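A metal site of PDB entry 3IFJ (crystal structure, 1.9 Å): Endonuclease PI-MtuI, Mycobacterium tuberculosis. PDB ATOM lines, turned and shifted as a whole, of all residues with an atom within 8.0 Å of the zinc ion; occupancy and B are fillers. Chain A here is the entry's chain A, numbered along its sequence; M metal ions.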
ATOM      1  N   VAL A  46     -10.930  20.383  28.688  1.00  0.00           N
ATOM      2  CA  VAL A  46     -10.049  20.422  29.851  1.00  0.00           C
ATOM      3  C   VAL A  46      -9.830  21.800  30.458  1.00  0.00           C
ATOM      4  O   VAL A  46      -9.221  21.918  31.524  1.00  0.00           O
ATOM      5  CB  VAL A  46      -8.667  19.807  29.531  1.00  0.00           C
ATOM      6  CG1 VAL A  46      -8.829  18.329  29.172  1.00  0.00           C
ATOM      7  CG2 VAL A  46      -8.016  20.568  28.382  1.00  0.00           C
ATOM      8  N   SER A  47     -10.307  22.834  29.788  1.00  0.00           N
ATOM      9  CA  SER A  47     -10.187  24.201  30.301  1.00  0.00           C
ATOM     10  C   SER A  47     -11.399  24.996  29.847  1.00  0.00           C
ATOM     11  O   SER A  47     -11.938  24.753  28.770  1.00  0.00           O
ATOM     12  CB  SER A  47      -8.923  24.884  29.772  1.00  0.00           C
ATOM     13  OG  SER A  47      -7.771  24.126  30.085  1.00  0.00           O
ATOM     14  N   PHE A  49     -12.956  29.098  29.608  1.00  0.00           N
ATOM     15  CA  PHE A  49     -12.629  30.504  29.712  1.00  0.00           C
ATOM     16  C   PHE A  49     -13.812  31.442  29.473  1.00  0.00           C
ATOM     17  O   PHE A  49     -14.563  31.275  28.515  1.00  0.00           O
ATOM     18  CB  PHE A  49     -11.501  30.883  28.738  1.00  0.00           C
ATOM     19  CG  PHE A  49     -10.209  30.174  29.012  1.00  0.00           C
ATOM     20  CD1 PHE A  49      -9.973  28.906  28.486  1.00  0.00           C
ATOM     21  CD2 PHE A  49      -9.231  30.764  29.803  1.00  0.00           C
ATOM     22  CE1 PHE A  49      -8.780  28.232  28.753  1.00  0.00           C
ATOM     23  CE2 PHE A  49      -8.039  30.103  30.082  1.00  0.00           C
ATOM     24  CZ  PHE A  49      -7.809  28.827  29.556  1.00  0.00           C
ATOM     25  N   ASP A 121     -14.216  30.559  25.543  1.00  0.00           N
ATOM     26  CA  ASP A 121     -13.227  29.673  24.958  1.00  0.00           C
ATOM     27  C   ASP A 121     -13.192  28.351  25.718  1.00  0.00           C
ATOM     28  O   ASP A 121     -13.423  28.309  26.928  1.00  0.00           O
ATOM     29  CB  ASP A 121     -11.825  30.306  24.996  1.00  0.00           C
ATOM     30  CG  ASP A 121     -11.341  30.751  23.635  1.00  0.00           C
ATOM     31  OD1 ASP A 121     -11.375  29.934  22.689  1.00  0.00           O
ATOM     32  OD2 ASP A 121     -10.914  31.920  23.511  1.00  0.00           O
ATOM     33  N   LEU A 122     -12.900  27.274  25.006  1.00  0.00           N
ATOM     34  CA  LEU A 122     -12.812  25.944  25.609  1.00  0.00           C
ATOM     35  C   LEU A 122     -11.510  25.307  25.132  1.00  0.00           C
ATOM     36  O   LEU A 122     -11.141  25.456  23.982  1.00  0.00           O
ATOM     37  CB  LEU A 122     -13.959  25.042  25.143  1.00  0.00           C
ATOM     38  CG  LEU A 122     -15.414  25.400  25.472  1.00  0.00           C
ATOM     39  CD1 LEU A 122     -16.313  24.295  24.910  1.00  0.00           C
ATOM     40  CD2 LEU A 122     -15.599  25.524  26.968  1.00  0.00           C
ATOM     41  N   GLU A 123     -10.827  24.621  26.033  1.00  0.00           N
ATOM     42  CA  GLU A 123      -9.614  23.909  25.647  1.00  0.00           C
ATOM     43  C   GLU A 123     -10.002  22.437  25.542  1.00  0.00           C
ATOM     44  O   GLU A 123     -10.595  21.878  26.466  1.00  0.00           O
ATOM     45  CB  GLU A 123      -8.494  24.089  26.673  1.00  0.00           C
ATOM     46  CG  GLU A 123      -7.689  25.380  26.486  1.00  0.00           C
ATOM     47  CD  GLU A 123      -7.066  25.488  25.105  1.00  0.00           C
ATOM     48  OE1 GLU A 123      -6.413  24.520  24.654  1.00  0.00           O
ATOM     49  OE2 GLU A 123      -7.236  26.545  24.460  1.00  0.00           O
ATOM     50  N   VAL A 124      -9.665  21.853  24.395  1.00  0.00           N
ATOM     51  CA  VAL A 124      -9.980  20.458  24.099  1.00  0.00           C
ATOM     52  C   VAL A 124      -8.705  19.621  24.159  1.00  0.00           C
ATOM     53  O   VAL A 124      -7.714  19.927  23.492  1.00  0.00           O
ATOM     54  CB  VAL A 124     -10.611  20.358  22.693  1.00  0.00           C
ATOM     55  CG1 VAL A 124     -11.015  18.930  22.381  1.00  0.00           C
ATOM     56  CG2 VAL A 124     -11.818  21.306  22.629  1.00  0.00           C
ATOM     57  N   GLU A 125      -8.746  18.564  24.956  1.00  0.00           N
ATOM     58  CA  GLU A 125      -7.587  17.695  25.134  1.00  0.00           C
ATOM     59  C   GLU A 125      -6.959  17.163  23.864  1.00  0.00           C
ATOM     60  O   GLU A 125      -7.646  16.636  22.981  1.00  0.00           O
ATOM     61  CB  GLU A 125      -7.951  16.511  26.038  1.00  0.00           C
ATOM     62  CG  GLU A 125      -6.853  15.466  26.163  1.00  0.00           C
ATOM     63  CD  GLU A 125      -7.313  14.222  26.908  1.00  0.00           C
ATOM     64  OE1 GLU A 125      -7.367  14.261  28.150  1.00  0.00           O
ATOM     65  OE2 GLU A 125      -7.634  13.220  26.231  1.00  0.00           O
ATOM     66  N   GLU A 126      -5.647  17.321  23.787  1.00  0.00           N
ATOM     67  CA  GLU A 126      -4.822  16.849  22.687  1.00  0.00           C
ATOM     68  C   GLU A 126      -4.961  17.502  21.327  1.00  0.00           C
ATOM     69  O   GLU A 126      -3.985  18.000  20.774  1.00  0.00           O
ATOM     70  CB  GLU A 126      -5.006  15.328  22.527  1.00  0.00           C
ATOM     71  CG  GLU A 126      -4.241  14.742  21.339  1.00  0.00           C
ATOM     72  CD  GLU A 126      -4.497  13.251  21.138  1.00  0.00           C
ATOM     73  OE1 GLU A 126      -5.668  12.832  21.101  1.00  0.00           O
ATOM     74  OE2 GLU A 126      -3.510  12.496  20.991  1.00  0.00           O
ATOM     75  N   LEU A 127      -6.163  17.525  20.777  1.00  0.00           N
ATOM     76  CA  LEU A 127      -6.374  18.057  19.430  1.00  0.00           C
ATOM     77  C   LEU A 127      -6.473  19.563  19.252  1.00  0.00           C
ATOM     78  O   LEU A 127      -6.260  20.072  18.146  1.00  0.00           O
ATOM     79  CB  LEU A 127      -7.581  17.354  18.800  1.00  0.00           C
ATOM     80  CG  LEU A 127      -7.410  15.830  18.747  1.00  0.00           C
ATOM     81  CD1 LEU A 127      -8.567  15.207  18.000  1.00  0.00           C
ATOM     82  CD2 LEU A 127      -6.084  15.481  18.078  1.00  0.00           C
ATOM     83  N   HIS A 128      -6.816  20.279  20.314  1.00  0.00           N
ATOM     84  CA  HIS A 128      -6.912  21.741  20.262  1.00  0.00           C
ATOM     85  C   HIS A 128      -7.855  22.314  19.201  1.00  0.00           C
ATOM     86  O   HIS A 128      -7.685  23.448  18.755  1.00  0.00           O
ATOM     87  CB  HIS A 128      -5.508  22.344  20.084  1.00  0.00           C
ATOM     88  CG  HIS A 128      -4.665  22.247  21.317  1.00  0.00           C
ATOM     89  ND1 HIS A 128      -4.791  23.127  22.366  1.00  0.00           N
ATOM     90  CD2 HIS A 128      -3.729  21.347  21.695  1.00  0.00           C
ATOM     91  CE1 HIS A 128      -3.982  22.768  23.341  1.00  0.00           C
ATOM     92  NE2 HIS A 128      -3.327  21.683  22.957  1.00  0.00           N
ATOM     93  N   THR A 129      -8.849  21.521  18.804  1.00  0.00           N
ATOM     94  CA  THR A 129      -9.843  21.966  17.836  1.00  0.00           C
ATOM     95  C   THR A 129     -11.212  21.521  18.351  1.00  0.00           C
ATOM     96  O   THR A 129     -11.307  20.661  19.235  1.00  0.00           O
ATOM     97  CB  THR A 129      -9.619  21.338  16.442  1.00  0.00           C
ATOM     98  OG1 THR A 129      -9.726  19.912  16.537  1.00  0.00           O
ATOM     99  CG2 THR A 129      -8.257  21.715  15.889  1.00  0.00           C
ATOM    100  N   HIS A 138     -10.757  26.582  15.652  1.00  0.00           N
ATOM    101  CA  HIS A 138      -9.564  26.431  16.462  1.00  0.00           C
ATOM    102  C   HIS A 138      -9.927  26.488  17.938  1.00  0.00           C
ATOM    103  O   HIS A 138     -10.789  27.264  18.348  1.00  0.00           O
ATOM    104  CB  HIS A 138      -8.573  27.544  16.087  1.00  0.00           C
ATOM    105  CG  HIS A 138      -7.214  27.380  16.688  1.00  0.00           C
ATOM    106  ND1 HIS A 138      -6.836  27.997  17.862  1.00  0.00           N
ATOM    107  CD2 HIS A 138      -6.131  26.690  16.257  1.00  0.00           C
ATOM    108  CE1 HIS A 138      -5.578  27.710  18.116  1.00  0.00           C
ATOM    109  NE2 HIS A 138      -5.126  26.910  17.166  1.00  0.00           N
ATOM    110  N1  SNN A 139      -7.673  25.243  21.650  1.00  0.00           N
ATOM    111  C   SNN A 139      -8.015  26.187  20.775  1.00  0.00           C
ATOM    112  CA  SNN A 139      -9.385  25.873  20.234  1.00  0.00           C
ATOM    113  N   SNN A 139      -9.293  25.679  18.779  1.00  0.00           N
ATOM    114  C4  SNN A 139      -9.789  24.577  20.948  1.00  0.00           C
ATOM    115  C5  SNN A 139      -8.594  24.273  21.832  1.00  0.00           C
ATOM    116  O   SNN A 139      -7.338  27.143  20.463  1.00  0.00           O
ATOM    117  O5  SNN A 139      -8.483  23.318  22.575  1.00  0.00           O
HETATM  118 ZN    ZN M   1      -5.864  24.893  22.672  1.00  0.00          ZN
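ND1 of His 128 is bound to the zinc ion (2.1 Å).
OE1 of Glu 123 binds the zinc ion.
The zinc ion is bound by N1 of SNN 139 (2.1 Å).
The zinc ion has three donor atoms within binding distance.
Slightly farther from the zinc ion lies the side-chain carboxylate (OE2) of Glu 123 (2.8 Å).
The backbone carbonyl oxygen of Glu 123 lies within hydrogen-bond range of the backbone NH of Val 46.
The backbone NH of Glu 123 is in hydrogen-bond range of the backbone carbonyl oxygen of Ser 47 (3.0 Å).
O5 of SNN 139 lies within hydrogen-bond range of the backbone NH of Val 124 (2.6 Å).
The nearest printed residue that does not touch the zinc ion is Val 124 (5.2 Å).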
